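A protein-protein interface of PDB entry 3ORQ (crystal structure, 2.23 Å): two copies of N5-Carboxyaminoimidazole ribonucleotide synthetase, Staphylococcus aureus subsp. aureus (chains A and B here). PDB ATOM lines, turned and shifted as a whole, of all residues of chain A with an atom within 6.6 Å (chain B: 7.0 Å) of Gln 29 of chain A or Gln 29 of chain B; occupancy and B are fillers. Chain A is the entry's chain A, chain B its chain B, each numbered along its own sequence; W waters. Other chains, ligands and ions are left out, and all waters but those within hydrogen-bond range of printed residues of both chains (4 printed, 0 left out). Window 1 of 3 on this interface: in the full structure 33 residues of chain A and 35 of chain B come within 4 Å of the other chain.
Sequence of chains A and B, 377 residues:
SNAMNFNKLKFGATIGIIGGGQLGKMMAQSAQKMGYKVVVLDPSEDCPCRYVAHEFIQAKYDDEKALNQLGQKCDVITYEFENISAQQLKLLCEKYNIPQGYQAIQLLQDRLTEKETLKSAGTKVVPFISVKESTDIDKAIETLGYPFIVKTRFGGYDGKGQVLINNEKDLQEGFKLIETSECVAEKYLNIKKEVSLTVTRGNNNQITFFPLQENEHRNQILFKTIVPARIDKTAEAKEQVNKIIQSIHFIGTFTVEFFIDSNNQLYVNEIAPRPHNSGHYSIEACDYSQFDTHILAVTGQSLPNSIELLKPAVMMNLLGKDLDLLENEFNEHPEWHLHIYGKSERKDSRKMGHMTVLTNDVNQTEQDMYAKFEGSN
Of the printed residues of chain B, Lys 25 of chain A touches Gln 32 (2.8 Å). Of chain B, only Gln 29 and Lys 33 come within 4 Å of Gln 29 of chain A. Printed residues of chain B within 4 Å of Gln 32 of chain A: Lys 25 and Val 52. Ile 17 of chain B touches none of the printed residues of chain A. Of chain A, only Gln 29 and Lys 33 come within 4 Å of Gln 29 of chain B. The nearest residue of chain B that does not touch Gln 29 of chain A is Gln 32 of chain B (4.2 Å). The nearest printed residue of chain A that does not touch Gln 32 of chain B is Gln 29 of chain A (4.2 Å).
N of Lys 25 of chain B is in hydrogen-bond range of SG of Cys 49 of chain B (3.7 Å). The backbone NH of Lys 25 of chain A lies close to the side-chain sulfur of Cys 49 of chain A (3.7 Å). The side-chain amide nitrogen (NE2) of Gln 32 of chain A lies within hydrogen-bond range of the backbone carbonyl oxygen (O) of Val 52 of chain A, at 2.8 Å. The side-chain amide nitrogen (NE2) of Gln 32 of chain B is in hydrogen-bond range of the backbone carbonyl oxygen (O) of Val 52 of chain B (2.8 Å). The side-chain amino group (NZ) of Lys 33 of chain B is in salt-bridge range of the side-chain carboxylate (OD1) of Asp 292 of chain B (2.8 Å). The side-chain amino group (NZ) of Lys 33 of chain A lies within salt-bridge range of the side-chain carboxylate (OD1) of Asp 292 of chain A.
Printed residues of chain B that touch a printed residue of chain A: Lys 25, Gln 29, Gln 32, Lys 33 and Val 52. Hydrophobic or aromatic side chains of chain B within 4 Å of the printed part of chain A: Val 52. Of the 16 printed residues of chain A, 6 touch a printed residue of chain B. Printed residues of chain A that touch a printed residue of chain B: Lys 25, Gln 29, Gln 32, Lys 33, Val 52 and His 339. Hydrophobic or aromatic side chains of chain A that line the printed part of chain B: Val 52 and His 339.
Among the printed residues, merely in contact across the chains: His 339 of chain A with Lys 33 of chain B (3.5 Å), Val 52 of chain A with Gln 32 of chain B (3.5 Å), Gln 32 of chain A with Val 52 of chain B (3.6 Å), Lys 33 of chain A with Gln 29 of chain B (3.7 Å) and Gln 29 of chain A with Lys 33 of chain B (3.9 Å).
Lys 25 of chain A touches Gln 32 of chain B, and with the chains exchanged Gln 32 of chain A touches Lys 25 of chain B. Gln 29 of chain A touches its own counterpart, Gln 29 of chain B. Gln 29 of chain A touches Lys 33 of chain B, and with the chains exchanged Lys 33 of chain A touches Gln 29 of chain B. Gln 32 of chain A touches Val 52 of chain B, and with the chains exchanged Val 52 of chain A touches Gln 32 of chain B.
Water W2 lies within hydrogen-bond range of NZ of Lys 25 of chain B (2.7 Å) and O of Lys 33 of chain A (2.9 Å). Water W3 bridges OE1 of Gln 32 of chain B (2.8 Å) and NZ of Lys 25 of chain A (2.9 Å). Water W1 bridges the side-chain amide oxygen of Gln 32 of chain A and the side-chain amino group of Lys 25 of chain B. Water W4 bridges O of Lys 33 of chain B (2.9 Å) and NZ of Lys 25 of chain A (2.9 Å).
The backbone carbonyl oxygen of Gln 32 of chain A lies within hydrogen-bond range of the side-chain amino group of Lys 25 of chain B, 2.8 Å away. The backbone carbonyl oxygen (O) of Gln 32 of chain B lies within hydrogen-bond range of the side-chain amino group (NZ) of Lys 25 of chain A, at 2.8 Å. OE1 of Gln 29 of chain A is in hydrogen-bond range of NE2 of Gln 29 of chain B.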
ATOM      1  N   GLY A  24      23.854   2.558  12.836  1.00  0.00           N
ATOM      2  CA  GLY A  24      24.042   3.972  13.122  1.00  0.00           C
ATOM      3  C   GLY A  24      23.510   4.790  11.959  1.00  0.00           C
ATOM      4  O   GLY A  24      22.843   5.815  12.157  1.00  0.00           O
ATOM      5  N   LYS A  25      23.736   4.306  10.741  1.00  0.00           N
ATOM      6  CA  LYS A  25      23.380   5.046   9.546  1.00  0.00           C
ATOM      7  C   LYS A  25      21.884   5.197   9.519  1.00  0.00           C
ATOM      8  O   LYS A  25      21.338   6.275   9.309  1.00  0.00           O
ATOM      9  CB  LYS A  25      23.855   4.268   8.287  1.00  0.00           C
ATOM     10  CG  LYS A  25      23.332   4.849   6.910  1.00  0.00           C
ATOM     11  CD  LYS A  25      23.708   3.954   5.694  1.00  0.00           C
ATOM     12  CE  LYS A  25      23.284   4.674   4.419  1.00  0.00           C
ATOM     13  NZ  LYS A  25      23.634   3.904   3.229  1.00  0.00           N
ATOM     14  N   MET A  26      21.186   4.107   9.740  1.00  0.00           N
ATOM     15  CA  MET A  26      19.738   4.167   9.677  1.00  0.00           C
ATOM     16  C   MET A  26      19.116   4.991  10.846  1.00  0.00           C
ATOM     17  O   MET A  26      18.082   5.654  10.670  1.00  0.00           O
ATOM     18  CB  MET A  26      19.202   2.752   9.589  1.00  0.00           C
ATOM     19  CG  MET A  26      19.596   2.041   8.279  1.00  0.00           C
ATOM     20  SD  MET A  26      18.795   0.236   8.141  1.00  0.00           S
ATOM     21  CE  MET A  26      20.170  -0.747   9.015  1.00  0.00           C
ATOM     22  N   MET A  27      19.747   4.956  12.019  1.00  0.00           N
ATOM     23  CA  MET A  27      19.356   5.803  13.134  1.00  0.00           C
ATOM     24  C   MET A  27      19.517   7.247  12.707  1.00  0.00           C
ATOM     25  O   MET A  27      18.648   8.067  13.011  1.00  0.00           O
ATOM     26  CB  MET A  27      20.313   5.610  14.331  1.00  0.00           C
ATOM     27  CG  MET A  27      20.108   4.352  15.196  1.00  0.00           C
ATOM     28  SD  MET A  27      21.364   4.327  16.706  1.00  0.00           S
ATOM     29  CE  MET A  27      20.968   2.563  17.401  1.00  0.00           C
ATOM     30  N   ALA A  28      20.655   7.568  12.071  1.00  0.00           N
ATOM     31  CA  ALA A  28      20.966   8.960  11.698  1.00  0.00           C
ATOM     32  C   ALA A  28      20.016   9.486  10.609  1.00  0.00           C
ATOM     33  O   ALA A  28      19.618  10.680  10.634  1.00  0.00           O
ATOM     34  CB  ALA A  28      22.455   9.103  11.234  1.00  0.00           C
ATOM     35  N   GLN A  29      19.637   8.603   9.669  1.00  0.00           N
ATOM     36  CA  GLN A  29      18.635   8.989   8.655  1.00  0.00           C
ATOM     37  C   GLN A  29      17.287   9.318   9.274  1.00  0.00           C
ATOM     38  O   GLN A  29      16.663  10.315   8.899  1.00  0.00           O
ATOM     39  CB  GLN A  29      18.509   7.945   7.551  1.00  0.00           C
ATOM     40  CG  GLN A  29      19.812   7.886   6.702  1.00  0.00           C
ATOM     41  CD  GLN A  29      19.648   7.105   5.387  1.00  0.00           C
ATOM     42  OE1 GLN A  29      19.329   7.687   4.381  1.00  0.00           O
ATOM     43  NE2 GLN A  29      19.813   5.772   5.430  1.00  0.00           N
ATOM     44  N   SER A  30      16.845   8.530  10.259  1.00  0.00           N
ATOM     45  CA  SER A  30      15.621   8.894  10.975  1.00  0.00           C
ATOM     46  C   SER A  30      15.780  10.207  11.745  1.00  0.00           C
ATOM     47  O   SER A  30      14.887  11.067  11.725  1.00  0.00           O
ATOM     48  CB  SER A  30      15.173   7.816  11.979  1.00  0.00           C
ATOM     49  OG  SER A  30      14.630   6.732  11.262  1.00  0.00           O
ATOM     50  N   ALA A  31      16.883  10.335  12.454  1.00  0.00           N
ATOM     51  CA  ALA A  31      17.130  11.531  13.239  1.00  0.00           C
ATOM     52  C   ALA A  31      17.114  12.771  12.348  1.00  0.00           C
ATOM     53  O   ALA A  31      16.509  13.779  12.721  1.00  0.00           O
ATOM     54  CB  ALA A  31      18.450  11.421  13.964  1.00  0.00           C
ATOM     55  N   GLN A  32      17.770  12.722  11.174  1.00  0.00           N
ATOM     56  CA  GLN A  32      17.802  13.932  10.304  1.00  0.00           C
ATOM     57  C   GLN A  32      16.426  14.257   9.719  1.00  0.00           C
ATOM     58  O   GLN A  32      15.985  15.411   9.709  1.00  0.00           O
ATOM     59  CB  GLN A  32      18.868  13.784   9.221  1.00  0.00           C
ATOM     60  CG  GLN A  32      20.286  14.062   9.785  1.00  0.00           C
ATOM     61  CD  GLN A  32      21.169  14.628   8.754  1.00  0.00           C
ATOM     62  OE1 GLN A  32      20.812  15.622   8.099  1.00  0.00           O
ATOM     63  NE2 GLN A  32      22.337  14.008   8.552  1.00  0.00           N
ATOM     64  N   LYS A  33      15.708  13.234   9.262  1.00  0.00           N
ATOM     65  CA  LYS A  33      14.306  13.398   8.892  1.00  0.00           C
ATOM     66  C   LYS A  33      13.448  14.160   9.973  1.00  0.00           C
ATOM     67  O   LYS A  33      12.667  15.015   9.627  1.00  0.00           O
ATOM     68  CB  LYS A  33      13.672  12.024   8.672  1.00  0.00           C
ATOM     69  CG  LYS A  33      12.141  12.086   8.512  1.00  0.00           C
ATOM     70  CD  LYS A  33      11.616  10.697   8.307  1.00  0.00           C
ATOM     71  CE  LYS A  33      11.809   9.835   9.565  1.00  0.00           C
ATOM     72  NZ  LYS A  33      11.179   8.506   9.387  1.00  0.00           N
ATOM     73  N   MET A  34      13.594  13.798  11.246  1.00  0.00           N
ATOM     74  CA  MET A  34      12.869  14.447  12.357  1.00  0.00           C
ATOM     75  C   MET A  34      13.458  15.795  12.775  1.00  0.00           C
ATOM     76  O   MET A  34      12.925  16.455  13.672  1.00  0.00           O
ATOM     77  CB  MET A  34      12.824  13.523  13.588  1.00  0.00           C
ATOM     78  CG  MET A  34      11.843  12.380  13.445  1.00  0.00           C
ATOM     79  SD  MET A  34      11.945  11.059  14.893  1.00  0.00           S
ATOM     80  CE  MET A  34      10.945   9.683  13.916  1.00  0.00           C
ATOM     81  N   VAL A  38      23.169  15.201  13.917  1.00  0.00           N
ATOM     82  CA  VAL A  38      23.795  13.935  14.268  1.00  0.00           C
ATOM     83  C   VAL A  38      25.301  14.076  14.280  1.00  0.00           C
ATOM     84  O   VAL A  38      25.888  14.495  13.286  1.00  0.00           O
ATOM     85  CB  VAL A  38      23.451  12.839  13.237  1.00  0.00           C
ATOM     86  CG1 VAL A  38      24.266  11.567  13.534  1.00  0.00           C
ATOM     87  CG2 VAL A  38      21.944  12.520  13.245  1.00  0.00           C
ATOM     88  N   CYS A  49      27.902   5.480   8.092  1.00  0.00           N
ATOM     89  CA  CYS A  49      27.078   6.549   8.694  1.00  0.00           C
ATOM     90  C   CYS A  49      27.729   7.927   8.471  1.00  0.00           C
ATOM     91  O   CYS A  49      27.125   8.962   8.722  1.00  0.00           O
ATOM     92  CB  CYS A  49      26.911   6.280  10.204  1.00  0.00           C
ATOM     93  SG  CYS A  49      25.792   7.409  11.143  1.00  0.00           S
ATOM     94  N   VAL A  52      25.743  10.724   6.595  1.00  0.00           N
ATOM     95  CA  VAL A  52      24.447  11.156   7.097  1.00  0.00           C
ATOM     96  C   VAL A  52      24.554  11.721   8.545  1.00  0.00           C
ATOM     97  O   VAL A  52      23.599  11.630   9.355  1.00  0.00           O
ATOM     98  CB  VAL A  52      23.432   9.996   7.005  1.00  0.00           C
ATOM     99  CG1 VAL A  52      23.084   9.718   5.559  1.00  0.00           C
ATOM    100  CG2 VAL A  52      23.953   8.741   7.676  1.00  0.00           C
ATOM    101  N   ASP A 292      12.874   4.842  13.916  1.00  0.00           N
ATOM    102  CA  ASP A 292      12.050   5.982  14.281  1.00  0.00           C
ATOM    103  C   ASP A 292      11.771   5.920  15.779  1.00  0.00           C
ATOM    104  O   ASP A 292      12.010   6.888  16.488  1.00  0.00           O
ATOM    105  CB  ASP A 292      10.708   5.983  13.538  1.00  0.00           C
ATOM    106  CG  ASP A 292      10.862   6.070  12.019  1.00  0.00           C
ATOM    107  OD1 ASP A 292      11.839   6.703  11.503  1.00  0.00           O
ATOM    108  OD2 ASP A 292       9.994   5.449  11.341  1.00  0.00           O
ATOM    109  N   HIS A 339      18.305  -1.973   0.063  1.00  0.00           N
ATOM    110  CA  HIS A 339      19.152  -1.122   0.925  1.00  0.00           C
ATOM    111  C   HIS A 339      20.607  -1.526   0.724  1.00  0.00           C
ATOM    112  O   HIS A 339      20.964  -2.684   0.959  1.00  0.00           O
ATOM    113  CB  HIS A 339      18.828  -1.352   2.412  1.00  0.00           C
ATOM    114  CG  HIS A 339      17.528  -0.769   2.838  1.00  0.00           C
ATOM    115  ND1 HIS A 339      17.438   0.245   3.771  1.00  0.00           N
ATOM    116  CD2 HIS A 339      16.261  -1.026   2.436  1.00  0.00           C
ATOM    117  CE1 HIS A 339      16.167   0.550   3.959  1.00  0.00           C
ATOM    118  NE2 HIS A 339      15.431  -0.188   3.148  1.00  0.00           N
ATOM    119  N   ILE B  17      22.671  16.704  -7.224  1.00  0.00           N
ATOM    120  CA  ILE B  17      21.409  17.387  -7.070  1.00  0.00           C
ATOM    121  C   ILE B  17      21.675  18.886  -7.127  1.00  0.00           C
ATOM    122  O   ILE B  17      22.500  19.392  -6.362  1.00  0.00           O
ATOM    123  CB  ILE B  17      20.771  17.076  -5.723  1.00  0.00           C
ATOM    124  CG1 ILE B  17      20.654  15.569  -5.519  1.00  0.00           C
ATOM    125  CG2 ILE B  17      19.416  17.763  -5.606  1.00  0.00           C
ATOM    126  CD1 ILE B  17      20.288  15.180  -4.070  1.00  0.00           C
ATOM    127  N   GLY B  24      15.512  18.290  -2.236  1.00  0.00           N
ATOM    128  CA  GLY B  24      16.820  17.661  -2.512  1.00  0.00           C
ATOM    129  C   GLY B  24      17.219  16.816  -1.289  1.00  0.00           C
ATOM    130  O   GLY B  24      17.761  15.725  -1.423  1.00  0.00           O
ATOM    131  N   LYS B  25      16.930  17.281  -0.073  1.00  0.00           N
ATOM    132  CA  LYS B  25      17.277  16.498   1.123  1.00  0.00           C
ATOM    133  C   LYS B  25      16.591  15.148   1.040  1.00  0.00           C
ATOM    134  O   LYS B  25      17.223  14.108   1.311  1.00  0.00           O
ATOM    135  CB  LYS B  25      16.799  17.202   2.411  1.00  0.00           C
ATOM    136  CG  LYS B  25      17.010  16.395   3.700  1.00  0.00           C
ATOM    137  CD  LYS B  25      16.398  17.152   4.934  1.00  0.00           C
ATOM    138  CE  LYS B  25      16.710  16.445   6.266  1.00  0.00           C
ATOM    139  NZ  LYS B  25      15.874  16.962   7.371  1.00  0.00           N
ATOM    140  N   MET B  26      15.277  15.151   0.738  1.00  0.00           N
ATOM    141  CA  MET B  26      14.547  13.893   0.726  1.00  0.00           C
ATOM    142  C   MET B  26      14.992  12.983  -0.461  1.00  0.00           C
ATOM    143  O   MET B  26      14.913  11.734  -0.384  1.00  0.00           O
ATOM    144  CB  MET B  26      13.037  14.123   0.752  1.00  0.00           C
ATOM    145  CG  MET B  26      12.545  14.653   2.103  1.00  0.00           C
ATOM    146  SD  MET B  26      10.658  15.048   2.159  1.00  0.00           S
ATOM    147  CE  MET B  26      10.724  16.842   1.719  1.00  0.00           C
ATOM    148  N   MET B  27      15.484  13.587  -1.532  1.00  0.00           N
ATOM    149  CA  MET B  27      16.083  12.777  -2.624  1.00  0.00           C
ATOM    150  C   MET B  27      17.355  12.111  -2.149  1.00  0.00           C
ATOM    151  O   MET B  27      17.616  10.955  -2.470  1.00  0.00           O
ATOM    152  CB  MET B  27      16.493  13.672  -3.811  1.00  0.00           C
ATOM    153  CG  MET B  27      15.303  14.252  -4.639  1.00  0.00           C
ATOM    154  SD  MET B  27      16.016  15.266  -6.120  1.00  0.00           S
ATOM    155  CE  MET B  27      14.389  15.740  -7.026  1.00  0.00           C
ATOM    156  N   ALA B  28      18.168  12.864  -1.412  1.00  0.00           N
ATOM    157  CA  ALA B  28      19.494  12.389  -1.014  1.00  0.00           C
ATOM    158  C   ALA B  28      19.337  11.239  -0.040  1.00  0.00           C
ATOM    159  O   ALA B  28      20.107  10.300  -0.089  1.00  0.00           O
ATOM    160  CB  ALA B  28      20.317  13.558  -0.391  1.00  0.00           C
ATOM    161  N   GLN B  29      18.345  11.323   0.848  1.00  0.00           N
ATOM    162  CA  GLN B  29      18.117  10.276   1.850  1.00  0.00           C
ATOM    163  C   GLN B  29      17.757   8.947   1.203  1.00  0.00           C
ATOM    164  O   GLN B  29      18.249   7.916   1.640  1.00  0.00           O
ATOM    165  CB  GLN B  29      17.015  10.705   2.845  1.00  0.00           C
ATOM    166  CG  GLN B  29      17.459  11.822   3.803  1.00  0.00           C
ATOM    167  CD  GLN B  29      17.568  11.333   5.183  1.00  0.00           C
ATOM    168  OE1 GLN B  29      16.959  11.873   6.100  1.00  0.00           O
ATOM    169  NE2 GLN B  29      18.364  10.253   5.361  1.00  0.00           N
ATOM    170  N   SER B  30      16.895   8.976   0.171  1.00  0.00           N
ATOM    171  CA  SER B  30      16.594   7.775  -0.629  1.00  0.00           C
ATOM    172  C   SER B  30      17.831   7.261  -1.375  1.00  0.00           C
ATOM    173  O   SER B  30      18.119   6.059  -1.360  1.00  0.00           O
ATOM    174  CB  SER B  30      15.505   8.056  -1.665  1.00  0.00           C
ATOM    175  OG  SER B  30      14.280   8.228  -1.017  1.00  0.00           O
ATOM    176  N   ALA B  31      18.568   8.170  -1.992  1.00  0.00           N
ATOM    177  CA  ALA B  31      19.782   7.821  -2.743  1.00  0.00           C
ATOM    178  C   ALA B  31      20.781   7.130  -1.813  1.00  0.00           C
ATOM    179  O   ALA B  31      21.308   6.055  -2.145  1.00  0.00           O
ATOM    180  CB  ALA B  31      20.407   9.058  -3.394  1.00  0.00           C
ATOM    181  N   GLN B  32      21.007   7.711  -0.639  1.00  0.00           N
ATOM    182  CA  GLN B  32      21.944   7.095   0.290  1.00  0.00           C
ATOM    183  C   GLN B  32      21.452   5.773   0.854  1.00  0.00           C
ATOM    184  O   GLN B  32      22.222   4.841   0.994  1.00  0.00           O
ATOM    185  CB  GLN B  32      22.327   8.058   1.395  1.00  0.00           C
ATOM    186  CG  GLN B  32      23.398   9.029   0.933  1.00  0.00           C
ATOM    187  CD  GLN B  32      24.246   9.434   2.067  1.00  0.00           C
ATOM    188  OE1 GLN B  32      24.829   8.571   2.768  1.00  0.00           O
ATOM    189  NE2 GLN B  32      24.308  10.742   2.311  1.00  0.00           N
ATOM    190  N   LYS B  33      20.150   5.695   1.142  1.00  0.00           N
ATOM    191  CA  LYS B  33      19.540   4.448   1.527  1.00  0.00           C
ATOM    192  C   LYS B  33      19.826   3.361   0.461  1.00  0.00           C
ATOM    193  O   LYS B  33      20.134   2.218   0.796  1.00  0.00           O
ATOM    194  CB  LYS B  33      18.037   4.631   1.738  1.00  0.00           C
ATOM    195  CG  LYS B  33      17.323   3.320   1.888  1.00  0.00           C
ATOM    196  CD  LYS B  33      15.806   3.505   1.997  1.00  0.00           C
ATOM    197  CE  LYS B  33      15.189   3.850   0.655  1.00  0.00           C
ATOM    198  NZ  LYS B  33      13.749   4.237   0.767  1.00  0.00           N
ATOM    199  N   MET B  34      19.761   3.739  -0.812  1.00  0.00           N
ATOM    200  CA  MET B  34      19.928   2.762  -1.908  1.00  0.00           C
ATOM    201  C   MET B  34      21.425   2.579  -2.341  1.00  0.00           C
ATOM    202  O   MET B  34      21.734   1.893  -3.292  1.00  0.00           O
ATOM    203  CB  MET B  34      19.079   3.226  -3.087  1.00  0.00           C
ATOM    204  CG  MET B  34      17.592   3.427  -2.712  1.00  0.00           C
ATOM    205  SD  MET B  34      16.540   4.533  -4.014  1.00  0.00           S
ATOM    206  CE  MET B  34      16.509   3.189  -5.261  1.00  0.00           C
ATOM    207  N   VAL B  38      26.016  11.127  -2.994  1.00  0.00           N
ATOM    208  CA  VAL B  38      25.290  12.340  -3.302  1.00  0.00           C
ATOM    209  C   VAL B  38      26.209  13.566  -3.261  1.00  0.00           C
ATOM    210  O   VAL B  38      26.889  13.814  -2.250  1.00  0.00           O
ATOM    211  CB  VAL B  38      24.115  12.557  -2.306  1.00  0.00           C
ATOM    212  CG1 VAL B  38      23.443  13.916  -2.584  1.00  0.00           C
ATOM    213  CG2 VAL B  38      23.104  11.412  -2.392  1.00  0.00           C
ATOM    214  N   CYS B  49      19.868  20.034   2.761  1.00  0.00           N
ATOM    215  CA  CYS B  49      20.381  18.802   2.141  1.00  0.00           C
ATOM    216  C   CYS B  49      21.860  18.602   2.496  1.00  0.00           C
ATOM    217  O   CYS B  49      22.418  17.550   2.241  1.00  0.00           O
ATOM    218  CB  CYS B  49      20.232  18.846   0.605  1.00  0.00           C
ATOM    219  SG  CYS B  49      20.618  17.258  -0.256  1.00  0.00           S
ATOM    220  N   VAL B  52      23.270  15.371   4.342  1.00  0.00           N
ATOM    221  CA  VAL B  52      23.002  14.045   3.814  1.00  0.00           C
ATOM    222  C   VAL B  52      23.611  13.903   2.430  1.00  0.00           C
ATOM    223  O   VAL B  52      23.064  13.199   1.579  1.00  0.00           O
ATOM    224  CB  VAL B  52      21.490  13.700   3.818  1.00  0.00           C
ATOM    225  CG1 VAL B  52      21.011  13.454   5.220  1.00  0.00           C
ATOM    226  CG2 VAL B  52      20.642  14.803   3.184  1.00  0.00           C
ATOM    227  N   ASP B 292      11.792   7.778  -3.678  1.00  0.00           N
ATOM    228  CA  ASP B 292      12.327   6.467  -4.047  1.00  0.00           C
ATOM    229  C   ASP B 292      12.180   6.214  -5.552  1.00  0.00           C
ATOM    230  O   ASP B 292      13.141   5.757  -6.202  1.00  0.00           O
ATOM    231  CB  ASP B 292      11.615   5.304  -3.366  1.00  0.00           C
ATOM    232  CG  ASP B 292      11.722   5.330  -1.889  1.00  0.00           C
ATOM    233  OD1 ASP B 292      12.739   5.829  -1.357  1.00  0.00           O
ATOM    234  OD2 ASP B 292      10.734   4.834  -1.264  1.00  0.00           O
ATOM    235  N   ILE B 295      14.612   8.373  -7.791  1.00  0.00           N
ATOM    236  CA  ILE B 295      15.970   7.856  -7.829  1.00  0.00           C
ATOM    237  C   ILE B 295      16.097   6.617  -8.762  1.00  0.00           C
ATOM    238  O   ILE B 295      17.032   6.536  -9.551  1.00  0.00           O
ATOM    239  CB  ILE B 295      16.474   7.470  -6.410  1.00  0.00           C
ATOM    240  CG1 ILE B 295      16.437   8.680  -5.484  1.00  0.00           C
ATOM    241  CG2 ILE B 295      17.935   6.787  -6.499  1.00  0.00           C
ATOM    242  CD1 ILE B 295      17.243   9.893  -6.020  1.00  0.00           C
HETATM  243  O   HOH W   1      18.769  17.486   8.615  1.00  0.00           O
HETATM  244  O   HOH W   2      13.231  16.452   7.189  1.00  0.00           O
HETATM  245  O   HOH W   3      25.274   5.939   1.946  1.00  0.00           O
HETATM  246  O   HOH W   4      21.612   1.827   3.244  1.00  0.00           O
